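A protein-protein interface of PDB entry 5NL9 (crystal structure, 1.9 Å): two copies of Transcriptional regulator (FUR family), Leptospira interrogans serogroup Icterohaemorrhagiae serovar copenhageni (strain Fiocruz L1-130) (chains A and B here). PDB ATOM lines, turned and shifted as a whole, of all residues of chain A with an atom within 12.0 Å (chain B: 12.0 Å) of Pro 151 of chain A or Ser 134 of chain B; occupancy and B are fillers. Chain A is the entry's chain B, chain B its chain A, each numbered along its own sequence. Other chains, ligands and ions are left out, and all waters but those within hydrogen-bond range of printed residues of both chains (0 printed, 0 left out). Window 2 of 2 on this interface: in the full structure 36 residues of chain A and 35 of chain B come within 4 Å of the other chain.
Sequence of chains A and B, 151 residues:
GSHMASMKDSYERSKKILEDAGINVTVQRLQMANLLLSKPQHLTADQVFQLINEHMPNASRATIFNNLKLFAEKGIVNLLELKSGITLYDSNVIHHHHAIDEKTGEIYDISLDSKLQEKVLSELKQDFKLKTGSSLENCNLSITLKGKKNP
The side-chain carboxylate (OE2) of Glu 137 of chain B sits close to the side-chain amide oxygen (OD1) of Asn 150 of chain A.
The backbone carbonyl oxygen (O) of Ser 135 of chain B lies within hydrogen-bond range of the backbone NH (N) of Asn 150 of chain A (3.0 Å).
The backbone carbonyl oxygen of Glu 137 of chain B sits at hydrogen-bond distance from the backbone NH of Lys 148 of chain A.
The backbone carbonyl oxygen of Ile 100 of chain A is in hydrogen-bond range of the backbone NH of Gly 147 of chain A, at 3.2 Å.
N of Ile 100 of chain A sits at hydrogen-bond distance from O of Leu 145 of chain A (2.8 Å).
The backbone carbonyl oxygen (O) of Ala 99 of chain A lies within hydrogen-bond range of the backbone NH (N) of Tyr 108 of chain A, at 2.8 Å.
The side-chain hydroxyl of Thr 132 of chain B lies within hydrogen-bond range of the backbone carbonyl oxygen of Phe 128 of chain B.
The side-chain carboxylate (OD1) of Asp 101 of chain A lies within hydrogen-bond range of the backbone NH (N) of Lys 149 of chain A (3.1 Å).
The side-chain hydroxyl (OH) of Tyr 108 of chain A lies within hydrogen-bond range of the side-chain amino group (NZ) of Lys 149 of chain A, 2.8 Å away.
Phe 128 of chain B touches Tyr 108 of chain A (CE1 to CG, 3.6 Å).
CB of Leu 124 of chain B touches CD2 of Leu 145 of chain A, at 3.9 Å.
Lys 125 of chain B touches Leu 145 of chain A (N to CD2, 3.996 Å).
Gly 147 of chain A touches Leu 136 of chain B (C to CD1, 3.8 Å).
Gly 147 of chain A touches Glu 137 of chain B (CA to O, 3.3 Å).
Gly 147 of chain A touches Asn 138 of chain B.
O of Lys 148 of chain A touches O of Ser 135 of chain B, 3.8 Å away.
CA of Leu 136 of chain B touches O of Lys 148 of chain A, 3.6 Å away.
Lys 149 of chain A touches Ser 135 of chain B (CA to O, 3.7 Å).
Pro 151 of chain A touches Ser 134 of chain B.
Pro 151 of chain A touches just one residue of chain B: Ser 134 (3.6 Å).
Ser 134 of chain B touches just these residues of chain A: Lys 149 (3.7 Å), Asn 150 (3.6 Å) and Pro 151 (3.6 Å).
Of chain B, only Ser 134, Ser 135 and Leu 136 come within 4 Å of Lys 149 of chain A.
Asn 150 of chain A touches just these residues of chain B: Ser 134 (3.6 Å), Ser 135 (3.0 Å) and Glu 137 (3.1 Å).
Of chain A, only Ala 99 (3.3 Å), Tyr 108 (3.6 Å) and Ile 110 (3.8 Å) come within 4 Å of Phe 128 of chain B.
No residue of chain A comes within 4 Å of Gly 133 of chain B.
Leu 136 of chain B touches five residues of chain A.
Of the printed residues of chain A, Glu 137 of chain B touches Gly 147 (3.3 Å), Lys 148 (2.8 Å) and Asn 150 (3.1 Å).
Printed residues of chain B within 4 Å of Gly 147 of chain A: Leu 136, Glu 137 and Asn 138.
Ser 122 of chain B touches none of the printed residues of chain A.
Ile 100 of chain A touches none of the printed residues of chain B.
The nearest residue of chain B that does not touch Pro 151 of chain A is Ser 135 of chain B (4.9 Å).
Of the 19 printed residues of chain A, 10 touch a printed residue of chain B.
Of the 19 printed residues of chain B, 12 touch a printed residue of chain A.
Hydrophobic or aromatic side chains of chain B within 4 Å of the printed part of chain A: Leu 121, Leu 124, Phe 128 and Leu 136.
Among the printed residues, 27 pairs touch across the chains.
No position is printed for both chains.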
ATOM      1  N   ALA A  99     -29.827   7.067 -21.499  1.00  0.00           N
ATOM      2  CA  ALA A  99     -28.444   7.105 -21.925  1.00  0.00           C
ATOM      3  C   ALA A  99     -28.355   8.305 -22.848  1.00  0.00           C
ATOM      4  O   ALA A  99     -29.256   8.542 -23.654  1.00  0.00           O
ATOM      5  CB  ALA A  99     -28.060   5.842 -22.675  1.00  0.00           C
ATOM      6  N   ILE A 100     -27.318   9.087 -22.685  1.00  0.00           N
ATOM      7  CA  ILE A 100     -27.130  10.280 -23.503  1.00  0.00           C
ATOM      8  C   ILE A 100     -25.825  10.113 -24.292  1.00  0.00           C
ATOM      9  O   ILE A 100     -24.784   9.818 -23.706  1.00  0.00           O
ATOM     10  CB  ILE A 100     -27.080  11.568 -22.627  1.00  0.00           C
ATOM     11  CG1 ILE A 100     -28.399  11.780 -21.835  1.00  0.00           C
ATOM     12  CG2 ILE A 100     -26.765  12.802 -23.495  1.00  0.00           C
ATOM     13  CD1 ILE A 100     -28.413  13.071 -20.979  1.00  0.00           C
ATOM     14  N   ASP A 101     -25.886  10.317 -25.612  1.00  0.00           N
ATOM     15  CA  ASP A 101     -24.678  10.263 -26.442  1.00  0.00           C
ATOM     16  C   ASP A 101     -24.035  11.640 -26.289  1.00  0.00           C
ATOM     17  O   ASP A 101     -24.551  12.600 -26.845  1.00  0.00           O
ATOM     18  CB  ASP A 101     -25.041   9.964 -27.915  1.00  0.00           C
ATOM     19  CG  ASP A 101     -23.863   9.954 -28.898  1.00  0.00           C
ATOM     20  OD1 ASP A 101     -22.687   9.944 -28.437  1.00  0.00           O
ATOM     21  OD2 ASP A 101     -24.116   9.892 -30.119  1.00  0.00           O
ATOM     22  N   GLU A 102     -22.999  11.736 -25.436  1.00  0.00           N
ATOM     23  CA  GLU A 102     -22.307  12.981 -25.067  1.00  0.00           C
ATOM     24  C   GLU A 102     -21.791  13.783 -26.266  1.00  0.00           C
ATOM     25  O   GLU A 102     -21.679  15.006 -26.174  1.00  0.00           O
ATOM     26  CB  GLU A 102     -21.195  12.726 -24.035  1.00  0.00           C
ATOM     27  CG  GLU A 102     -20.014  11.894 -24.515  1.00  0.00           C
ATOM     28  CD  GLU A 102     -19.074  11.395 -23.435  1.00  0.00           C
ATOM     29  OE1 GLU A 102     -19.452  11.414 -22.241  1.00  0.00           O
ATOM     30  OE2 GLU A 102     -17.960  10.948 -23.793  1.00  0.00           O
ATOM     31  N   LYS A 103     -21.531  13.103 -27.393  1.00  0.00           N
ATOM     32  CA  LYS A 103     -21.107  13.748 -28.621  1.00  0.00           C
ATOM     33  C   LYS A 103     -22.271  14.538 -29.252  1.00  0.00           C
ATOM     34  O   LYS A 103     -22.180  15.766 -29.339  1.00  0.00           O
ATOM     35  CB  LYS A 103     -20.513  12.717 -29.602  1.00  0.00           C
ATOM     36  CG  LYS A 103     -19.059  12.357 -29.300  1.00  0.00           C
ATOM     37  CD  LYS A 103     -18.555  11.230 -30.205  1.00  0.00           C
ATOM     38  CE  LYS A 103     -17.050  11.106 -30.211  1.00  0.00           C
ATOM     39  NZ  LYS A 103     -16.406  12.170 -31.029  1.00  0.00           N
ATOM     40  N   THR A 104     -23.380  13.854 -29.615  1.00  0.00           N
ATOM     41  CA  THR A 104     -24.519  14.468 -30.305  1.00  0.00           C
ATOM     42  C   THR A 104     -25.575  15.115 -29.409  1.00  0.00           C
ATOM     43  O   THR A 104     -26.383  15.911 -29.885  1.00  0.00           O
ATOM     44  CB  THR A 104     -25.191  13.440 -31.223  1.00  0.00           C
ATOM     45  OG1 THR A 104     -25.731  12.388 -30.426  1.00  0.00           O
ATOM     46  CG2 THR A 104     -24.244  12.872 -32.266  1.00  0.00           C
ATOM     47  N   GLY A 105     -25.610  14.723 -28.146  1.00  0.00           N
ATOM     48  CA  GLY A 105     -26.618  15.184 -27.196  1.00  0.00           C
ATOM     49  C   GLY A 105     -27.908  14.383 -27.271  1.00  0.00           C
ATOM     50  O   GLY A 105     -28.858  14.667 -26.537  1.00  0.00           O
ATOM     51  N   GLU A 106     -27.952  13.383 -28.154  1.00  0.00           N
ATOM     52  CA  GLU A 106     -29.100  12.506 -28.356  1.00  0.00           C
ATOM     53  C   GLU A 106     -29.362  11.640 -27.115  1.00  0.00           C
ATOM     54  O   GLU A 106     -28.420  11.138 -26.495  1.00  0.00           O
ATOM     55  CB  GLU A 106     -28.887  11.609 -29.588  1.00  0.00           C
ATOM     56  CG  GLU A 106     -29.012  12.331 -30.928  1.00  0.00           C
ATOM     57  CD  GLU A 106     -30.414  12.513 -31.492  1.00  0.00           C
ATOM     58  OE1 GLU A 106     -31.020  11.498 -31.902  1.00  0.00           O
ATOM     59  OE2 GLU A 106     -30.815  13.682 -31.705  1.00  0.00           O
ATOM     60  N   ILE A 107     -30.644  11.457 -26.786  1.00  0.00           N
ATOM     61  CA  ILE A 107     -31.105  10.729 -25.608  1.00  0.00           C
ATOM     62  C   ILE A 107     -31.814   9.427 -25.994  1.00  0.00           C
ATOM     63  O   ILE A 107     -32.692   9.430 -26.860  1.00  0.00           O
ATOM     64  CB  ILE A 107     -32.028  11.666 -24.792  1.00  0.00           C
ATOM     65  CG1 ILE A 107     -31.301  12.931 -24.347  1.00  0.00           C
ATOM     66  CG2 ILE A 107     -32.688  10.961 -23.621  1.00  0.00           C
ATOM     67  CD1 ILE A 107     -32.224  14.169 -24.335  1.00  0.00           C
ATOM     68  N   TYR A 108     -31.456   8.324 -25.306  1.00  0.00           N
ATOM     69  CA  TYR A 108     -32.014   6.982 -25.508  1.00  0.00           C
ATOM     70  C   TYR A 108     -32.663   6.456 -24.236  1.00  0.00           C
ATOM     71  O   TYR A 108     -32.060   6.529 -23.169  1.00  0.00           O
ATOM     72  CB  TYR A 108     -30.910   6.004 -25.955  1.00  0.00           C
ATOM     73  CG  TYR A 108     -30.199   6.465 -27.206  1.00  0.00           C
ATOM     74  CD1 TYR A 108     -29.193   7.423 -27.144  1.00  0.00           C
ATOM     75  CD2 TYR A 108     -30.600   6.015 -28.463  1.00  0.00           C
ATOM     76  CE1 TYR A 108     -28.600   7.918 -28.299  1.00  0.00           C
ATOM     77  CE2 TYR A 108     -30.028   6.520 -29.632  1.00  0.00           C
ATOM     78  CZ  TYR A 108     -29.003   7.446 -29.544  1.00  0.00           C
ATOM     79  OH  TYR A 108     -28.379   7.891 -30.680  1.00  0.00           O
ATOM     80  N   ASP A 109     -33.860   5.872 -24.358  1.00  0.00           N
ATOM     81  CA  ASP A 109     -34.566   5.271 -23.229  1.00  0.00           C
ATOM     82  C   ASP A 109     -33.927   3.928 -22.910  1.00  0.00           C
ATOM     83  O   ASP A 109     -33.601   3.175 -23.821  1.00  0.00           O
ATOM     84  CB  ASP A 109     -36.043   5.065 -23.597  1.00  0.00           C
ATOM     85  CG  ASP A 109     -36.856   6.337 -23.565  1.00  0.00           C
ATOM     86  OD1 ASP A 109     -36.314   7.378 -23.100  1.00  0.00           O
ATOM     87  OD2 ASP A 109     -38.072   6.278 -23.900  1.00  0.00           O
ATOM     88  N   ILE A 110     -33.674   3.660 -21.623  1.00  0.00           N
ATOM     89  CA  ILE A 110     -33.055   2.415 -21.154  1.00  0.00           C
ATOM     90  C   ILE A 110     -33.702   2.016 -19.832  1.00  0.00           C
ATOM     91  O   ILE A 110     -34.205   2.888 -19.134  1.00  0.00           O
ATOM     92  CB  ILE A 110     -31.498   2.452 -21.122  1.00  0.00           C
ATOM     93  CG1 ILE A 110     -30.927   3.593 -20.239  1.00  0.00           C
ATOM     94  CG2 ILE A 110     -30.888   2.468 -22.521  1.00  0.00           C
ATOM     95  CD1 ILE A 110     -29.370   3.450 -19.956  1.00  0.00           C
ATOM     96  N   LEU A 145     -26.994   7.754 -17.955  1.00  0.00           N
ATOM     97  CA  LEU A 145     -25.729   7.134 -18.325  1.00  0.00           C
ATOM     98  C   LEU A 145     -25.220   7.996 -19.476  1.00  0.00           C
ATOM     99  O   LEU A 145     -25.922   8.167 -20.470  1.00  0.00           O
ATOM    100  CB  LEU A 145     -26.012   5.697 -18.775  1.00  0.00           C
ATOM    101  CG  LEU A 145     -24.846   4.868 -19.221  1.00  0.00           C
ATOM    102  CD1 LEU A 145     -24.015   4.513 -18.056  1.00  0.00           C
ATOM    103  CD2 LEU A 145     -25.308   3.578 -19.850  1.00  0.00           C
ATOM    104  N   LYS A 146     -24.059   8.624 -19.310  1.00  0.00           N
ATOM    105  CA  LYS A 146     -23.519   9.538 -20.326  1.00  0.00           C
ATOM    106  C   LYS A 146     -22.202   8.978 -20.893  1.00  0.00           C
ATOM    107  O   LYS A 146     -21.291   8.635 -20.140  1.00  0.00           O
ATOM    108  CB  LYS A 146     -23.332  10.924 -19.706  1.00  0.00           C
ATOM    109  CG  LYS A 146     -23.125  12.072 -20.690  1.00  0.00           C
ATOM    110  CD  LYS A 146     -23.859  13.377 -20.263  1.00  0.00           C
ATOM    111  CE  LYS A 146     -23.723  13.822 -18.811  1.00  0.00           C
ATOM    112  NZ  LYS A 146     -22.329  14.196 -18.443  1.00  0.00           N
ATOM    113  N   GLY A 147     -22.168   8.798 -22.208  1.00  0.00           N
ATOM    114  CA  GLY A 147     -21.005   8.233 -22.886  1.00  0.00           C
ATOM    115  C   GLY A 147     -20.971   8.520 -24.374  1.00  0.00           C
ATOM    116  O   GLY A 147     -21.820   9.249 -24.888  1.00  0.00           O
ATOM    117  N   LYS A 148     -19.994   7.936 -25.077  1.00  0.00           N
ATOM    118  CA  LYS A 148     -19.845   8.118 -26.527  1.00  0.00           C
ATOM    119  C   LYS A 148     -20.420   6.903 -27.263  1.00  0.00           C
ATOM    120  O   LYS A 148     -20.002   5.768 -27.022  1.00  0.00           O
ATOM    121  CB  LYS A 148     -18.364   8.337 -26.884  1.00  0.00           C
ATOM    122  N   LYS A 149     -21.450   7.137 -28.073  1.00  0.00           N
ATOM    123  CA  LYS A 149     -22.099   6.053 -28.822  1.00  0.00           C
ATOM    124  C   LYS A 149     -21.170   5.595 -29.945  1.00  0.00           C
ATOM    125  O   LYS A 149     -20.715   6.421 -30.742  1.00  0.00           O
ATOM    126  CB  LYS A 149     -23.461   6.520 -29.357  1.00  0.00           C
ATOM    127  CG  LYS A 149     -24.300   5.464 -30.059  1.00  0.00           C
ATOM    128  CD  LYS A 149     -25.445   6.133 -30.831  1.00  0.00           C
ATOM    129  CE  LYS A 149     -26.223   5.179 -31.715  1.00  0.00           C
ATOM    130  NZ  LYS A 149     -27.412   5.836 -32.341  1.00  0.00           N
ATOM    131  N   ASN A 150     -20.863   4.289 -29.968  1.00  0.00           N
ATOM    132  CA  ASN A 150     -20.002   3.682 -30.972  1.00  0.00           C
ATOM    133  C   ASN A 150     -20.646   2.399 -31.563  1.00  0.00           C
ATOM    134  O   ASN A 150     -20.829   1.440 -30.815  1.00  0.00           O
ATOM    135  CB  ASN A 150     -18.632   3.403 -30.381  1.00  0.00           C
ATOM    136  CG  ASN A 150     -17.689   2.719 -31.333  1.00  0.00           C
ATOM    137  OD1 ASN A 150     -17.130   1.668 -31.032  1.00  0.00           O
ATOM    138  ND2 ASN A 150     -17.522   3.279 -32.518  1.00  0.00           N
ATOM    139  N   PRO A 151     -21.036   2.327 -32.862  1.00  0.00           N
ATOM    140  CA  PRO A 151     -20.913   3.326 -33.956  1.00  0.00           C
ATOM    141  C   PRO A 151     -21.781   4.572 -33.754  1.00  0.00           C
ATOM    142  O   PRO A 151     -22.881   4.437 -33.188  1.00  0.00           O
ATOM    143  CB  PRO A 151     -21.416   2.557 -35.193  1.00  0.00           C
ATOM    144  CG  PRO A 151     -21.339   1.121 -34.837  1.00  0.00           C
ATOM    145  CD  PRO A 151     -21.629   1.073 -33.364  1.00  0.00           C
ATOM    146  OXT PRO A 151     -21.382   5.670 -34.201  1.00  0.00           O
ATOM    147  N   LEU B 121     -23.956   0.394 -13.762  1.00  0.00           N
ATOM    148  CA  LEU B 121     -23.323   0.893 -14.979  1.00  0.00           C
ATOM    149  C   LEU B 121     -23.234  -0.260 -16.029  1.00  0.00           C
ATOM    150  O   LEU B 121     -23.655  -0.074 -17.156  1.00  0.00           O
ATOM    151  CB  LEU B 121     -21.920   1.439 -14.660  1.00  0.00           C
ATOM    152  CG  LEU B 121     -21.171   2.094 -15.819  1.00  0.00           C
ATOM    153  CD1 LEU B 121     -21.553   3.554 -15.953  1.00  0.00           C
ATOM    154  CD2 LEU B 121     -19.677   2.042 -15.582  1.00  0.00           C
ATOM    155  N   SER B 122     -22.765  -1.452 -15.629  1.00  0.00           N
ATOM    156  CA  SER B 122     -22.707  -2.585 -16.543  1.00  0.00           C
ATOM    157  C   SER B 122     -24.086  -2.976 -17.102  1.00  0.00           C
ATOM    158  O   SER B 122     -24.170  -3.193 -18.299  1.00  0.00           O
ATOM    159  CB  SER B 122     -22.106  -3.794 -15.848  1.00  0.00           C
ATOM    160  OG  SER B 122     -21.565  -4.658 -16.829  1.00  0.00           O
ATOM    161  N   GLU B 123     -25.139  -3.154 -16.243  1.00  0.00           N
ATOM    162  CA  GLU B 123     -26.481  -3.559 -16.714  1.00  0.00           C
ATOM    163  C   GLU B 123     -27.066  -2.531 -17.641  1.00  0.00           C
ATOM    164  O   GLU B 123     -27.625  -2.886 -18.683  1.00  0.00           O
ATOM    165  CB  GLU B 123     -27.440  -3.893 -15.558  1.00  0.00           C
ATOM    166  CG  GLU B 123     -26.941  -5.103 -14.768  1.00  0.00           C
ATOM    167  CD  GLU B 123     -27.930  -6.046 -14.102  1.00  0.00           C
ATOM    168  OE1 GLU B 123     -29.148  -5.948 -14.376  1.00  0.00           O
ATOM    169  OE2 GLU B 123     -27.480  -6.890 -13.295  1.00  0.00           O
ATOM    170  N   LEU B 124     -26.869  -1.252 -17.328  1.00  0.00           N
ATOM    171  CA  LEU B 124     -27.397  -0.218 -18.203  1.00  0.00           C
ATOM    172  C   LEU B 124     -26.684  -0.210 -19.545  1.00  0.00           C
ATOM    173  O   LEU B 124     -27.338  -0.006 -20.567  1.00  0.00           O
ATOM    174  CB  LEU B 124     -27.367   1.151 -17.549  1.00  0.00           C
ATOM    175  CG  LEU B 124     -28.385   1.380 -16.420  1.00  0.00           C
ATOM    176  CD1 LEU B 124     -28.087   2.634 -15.724  1.00  0.00           C
ATOM    177  CD2 LEU B 124     -29.834   1.467 -16.945  1.00  0.00           C
ATOM    178  N   LYS B 125     -25.370  -0.407 -19.567  1.00  0.00           N
ATOM    179  CA  LYS B 125     -24.645  -0.467 -20.871  1.00  0.00           C
ATOM    180  C   LYS B 125     -25.167  -1.654 -21.710  1.00  0.00           C
ATOM    181  O   LYS B 125     -25.315  -1.527 -22.915  1.00  0.00           O
ATOM    182  CB  LYS B 125     -23.141  -0.679 -20.658  1.00  0.00           C
ATOM    183  CG  LYS B 125     -22.355   0.550 -20.264  1.00  0.00           C
ATOM    184  CD  LYS B 125     -20.853   0.163 -20.179  1.00  0.00           C
ATOM    185  CE  LYS B 125     -20.041   1.096 -19.325  1.00  0.00           C
ATOM    186  NZ  LYS B 125     -18.651   0.609 -19.133  1.00  0.00           N
ATOM    187  N   GLN B 126     -25.483  -2.797 -21.054  1.00  0.00           N
ATOM    188  CA  GLN B 126     -26.005  -3.961 -21.774  1.00  0.00           C
ATOM    189  C   GLN B 126     -27.374  -3.671 -22.339  1.00  0.00           C
ATOM    190  O   GLN B 126     -27.636  -4.033 -23.484  1.00  0.00           O
ATOM    191  CB  GLN B 126     -26.044  -5.218 -20.889  1.00  0.00           C
ATOM    192  CG  GLN B 126     -24.660  -5.743 -20.437  1.00  0.00           C
ATOM    193  CD  GLN B 126     -23.408  -5.244 -21.160  1.00  0.00           C
ATOM    194  OE1 GLN B 126     -23.115  -5.624 -22.307  1.00  0.00           O
ATOM    195  NE2 GLN B 126     -22.589  -4.434 -20.473  1.00  0.00           N
ATOM    196  N   ASP B 127     -28.229  -2.984 -21.581  1.00  0.00           N
ATOM    197  CA  ASP B 127     -29.558  -2.606 -22.073  1.00  0.00           C
ATOM    198  C   ASP B 127     -29.459  -1.593 -23.217  1.00  0.00           C
ATOM    199  O   ASP B 127     -30.258  -1.657 -24.155  1.00  0.00           O
ATOM    200  CB  ASP B 127     -30.433  -2.045 -20.949  1.00  0.00           C
ATOM    201  CG  ASP B 127     -31.918  -2.122 -21.273  1.00  0.00           C
ATOM    202  OD1 ASP B 127     -32.416  -3.246 -21.535  1.00  0.00           O
ATOM    203  OD2 ASP B 127     -32.590  -1.062 -21.274  1.00  0.00           O
ATOM    204  N   PHE B 128     -28.497  -0.640 -23.132  1.00  0.00           N
ATOM    205  CA  PHE B 128     -28.285   0.321 -24.210  1.00  0.00           C
ATOM    206  C   PHE B 128     -27.938  -0.452 -25.498  1.00  0.00           C
ATOM    207  O   PHE B 128     -28.520  -0.200 -26.559  1.00  0.00           O
ATOM    208  CB  PHE B 128     -27.154   1.286 -23.842  1.00  0.00           C
ATOM    209  CG  PHE B 128     -26.916   2.328 -24.916  1.00  0.00           C
ATOM    210  CD1 PHE B 128     -27.698   3.471 -24.981  1.00  0.00           C
ATOM    211  CD2 PHE B 128     -25.992   2.109 -25.921  1.00  0.00           C
ATOM    212  CE1 PHE B 128     -27.485   4.432 -25.972  1.00  0.00           C
ATOM    213  CE2 PHE B 128     -25.794   3.059 -26.922  1.00  0.00           C
ATOM    214  CZ  PHE B 128     -26.547   4.215 -26.941  1.00  0.00           C
ATOM    215  N   LYS B 129     -27.005  -1.404 -25.383  1.00  0.00           N
ATOM    216  CA  LYS B 129     -26.513  -2.231 -26.494  1.00  0.00           C
ATOM    217  C   LYS B 129     -27.676  -3.034 -27.088  1.00  0.00           C
ATOM    218  O   LYS B 129     -27.828  -3.067 -28.295  1.00  0.00           O
ATOM    219  CB  LYS B 129     -25.396  -3.160 -25.970  1.00  0.00           C
ATOM    220  CG  LYS B 129     -24.809  -4.135 -26.991  1.00  0.00           C
ATOM    221  CD  LYS B 129     -23.453  -3.663 -27.498  1.00  0.00           C
ATOM    222  CE  LYS B 129     -22.827  -4.644 -28.460  1.00  0.00           C
ATOM    223  NZ  LYS B 129     -22.026  -5.684 -27.755  1.00  0.00           N
ATOM    224  N   LEU B 130     -28.508  -3.648 -26.245  1.00  0.00           N
ATOM    225  CA  LEU B 130     -29.655  -4.435 -26.706  1.00  0.00           C
ATOM    226  C   LEU B 130     -30.677  -3.569 -27.466  1.00  0.00           C
ATOM    227  O   LEU B 130     -31.127  -3.960 -28.537  1.00  0.00           O
ATOM    228  CB  LEU B 130     -30.314  -5.169 -25.538  1.00  0.00           C
ATOM    229  CG  LEU B 130     -31.561  -6.000 -25.827  1.00  0.00           C
ATOM    230  CD1 LEU B 130     -31.277  -7.123 -26.842  1.00  0.00           C
ATOM    231  CD2 LEU B 130     -32.062  -6.624 -24.573  1.00  0.00           C
ATOM    232  N   LYS B 131     -30.986  -2.382 -26.945  1.00  0.00           N
ATOM    233  CA  LYS B 131     -31.940  -1.453 -27.550  1.00  0.00           C
ATOM    234  C   LYS B 131     -31.449  -0.742 -28.827  1.00  0.00           C
ATOM    235  O   LYS B 131     -32.267  -0.463 -29.704  1.00  0.00           O
ATOM    236  CB  LYS B 131     -32.369  -0.399 -26.514  1.00  0.00           C
ATOM    237  CG  LYS B 131     -33.731  -0.625 -25.902  1.00  0.00           C
ATOM    238  CD  LYS B 131     -33.597  -1.244 -24.549  1.00  0.00           C
ATOM    239  CE  LYS B 131     -34.894  -1.155 -23.813  1.00  0.00           C
ATOM    240  NZ  LYS B 131     -34.858  -1.962 -22.581  1.00  0.00           N
ATOM    241  N   THR B 132     -30.165  -0.383 -28.915  1.00  0.00           N
ATOM    242  CA  THR B 132     -29.687   0.399 -30.054  1.00  0.00           C
ATOM    243  C   THR B 132     -28.810  -0.377 -31.022  1.00  0.00           C
ATOM    244  O   THR B 132     -28.537   0.101 -32.122  1.00  0.00           O
ATOM    245  CB  THR B 132     -28.898   1.624 -29.551  1.00  0.00           C
ATOM    246  OG1 THR B 132     -27.670   1.170 -28.968  1.00  0.00           O
ATOM    247  CG2 THR B 132     -29.680   2.469 -28.554  1.00  0.00           C
ATOM    248  N   GLY B 133     -28.262  -1.490 -30.562  1.00  0.00           N
ATOM    249  CA  GLY B 133     -27.286  -2.252 -31.333  1.00  0.00           C
ATOM    250  C   GLY B 133     -25.878  -1.667 -31.245  1.00  0.00           C
ATOM    251  O   GLY B 133     -24.942  -2.238 -31.804  1.00  0.00           O
ATOM    252  N   SER B 134     -25.693  -0.540 -30.514  1.00  0.00           N
ATOM    253  CA  SER B 134     -24.374   0.096 -30.353  1.00  0.00           C
ATOM    254  C   SER B 134     -23.907   0.049 -28.903  1.00  0.00           C
ATOM    255  O   SER B 134     -24.723  -0.064 -27.996  1.00  0.00           O
ATOM    256  CB  SER B 134     -24.413   1.561 -30.795  1.00  0.00           C
ATOM    257  OG  SER B 134     -24.953   1.754 -32.087  1.00  0.00           O
ATOM    258  N   SER B 135     -22.602   0.197 -28.672  1.00  0.00           N
ATOM    259  CA  SER B 135     -22.086   0.202 -27.320  1.00  0.00           C
ATOM    260  C   SER B 135     -21.909   1.659 -26.892  1.00  0.00           C
ATOM    261  O   SER B 135     -21.784   2.543 -27.743  1.00  0.00           O
ATOM    262  CB  SER B 135     -20.762  -0.543 -27.260  1.00  0.00           C
ATOM    263  OG  SER B 135     -19.772   0.211 -27.943  1.00  0.00           O
ATOM    264  N   LEU B 136     -21.973   1.922 -25.583  1.00  0.00           N
ATOM    265  CA  LEU B 136     -21.772   3.265 -25.044  1.00  0.00           C
ATOM    266  C   LEU B 136     -20.409   3.237 -24.376  1.00  0.00           C
ATOM    267  O   LEU B 136     -20.147   2.367 -23.543  1.00  0.00           O
ATOM    268  CB  LEU B 136     -22.907   3.657 -24.080  1.00  0.00           C
ATOM    269  CG  LEU B 136     -23.144   5.162 -23.860  1.00  0.00           C
ATOM    270  CD1 LEU B 136     -23.577   5.875 -25.135  1.00  0.00           C
ATOM    271  CD2 LEU B 136     -24.218   5.381 -22.838  1.00  0.00           C
ATOM    272  N   GLU B 137     -19.503   4.087 -24.824  1.00  0.00           N
ATOM    273  CA  GLU B 137     -18.132   4.038 -24.326  1.00  0.00           C
ATOM    274  C   GLU B 137     -17.792   5.192 -23.403  1.00  0.00           C
ATOM    275  O   GLU B 137     -18.381   6.266 -23.538  1.00  0.00           O
ATOM    276  CB  GLU B 137     -17.141   3.966 -25.508  1.00  0.00           C
ATOM    277  CG  GLU B 137     -17.542   2.957 -26.578  1.00  0.00           C
ATOM    278  CD  GLU B 137     -16.537   2.647 -27.673  1.00  0.00           C
ATOM    279  OE1 GLU B 137     -15.999   3.598 -28.291  1.00  0.00           O
ATOM    280  OE2 GLU B 137     -16.379   1.444 -27.989  1.00  0.00           O
ATOM    281  N   ASN B 138     -16.818   4.960 -22.489  1.00  0.00           N
ATOM    282  CA  ASN B 138     -16.295   5.933 -21.510  1.00  0.00           C
ATOM    283  C   ASN B 138     -17.447   6.599 -20.736  1.00  0.00           C
ATOM    284  O   ASN B 138     -17.643   7.819 -20.767  1.00  0.00           O
ATOM    285  CB  ASN B 138     -15.344   6.939 -22.180  1.00  0.00           C
ATOM    286  CG  ASN B 138     -14.177   6.300 -22.923  1.00  0.00           C
ATOM    287  OD1 ASN B 138     -13.632   5.245 -22.541  1.00  0.00           O
ATOM    288  ND2 ASN B 138     -13.754   6.945 -24.005  1.00  0.00           N
ATOM    289  N   CYS B 139     -18.257   5.740 -20.116  1.00  0.00           N
ATOM    290  CA  CYS B 139     -19.465   6.098 -19.380  1.00  0.00           C
ATOM    291  C   CYS B 139     -19.264   6.659 -17.994  1.00  0.00           C
ATOM    292  O   CYS B 139     -18.509   6.099 -17.193  1.00  0.00           O
ATOM    293  CB  CYS B 139     -20.402   4.898 -19.298  1.00  0.00           C
ATOM    294  SG  CYS B 139     -20.945   4.279 -20.894  1.00  0.00           S
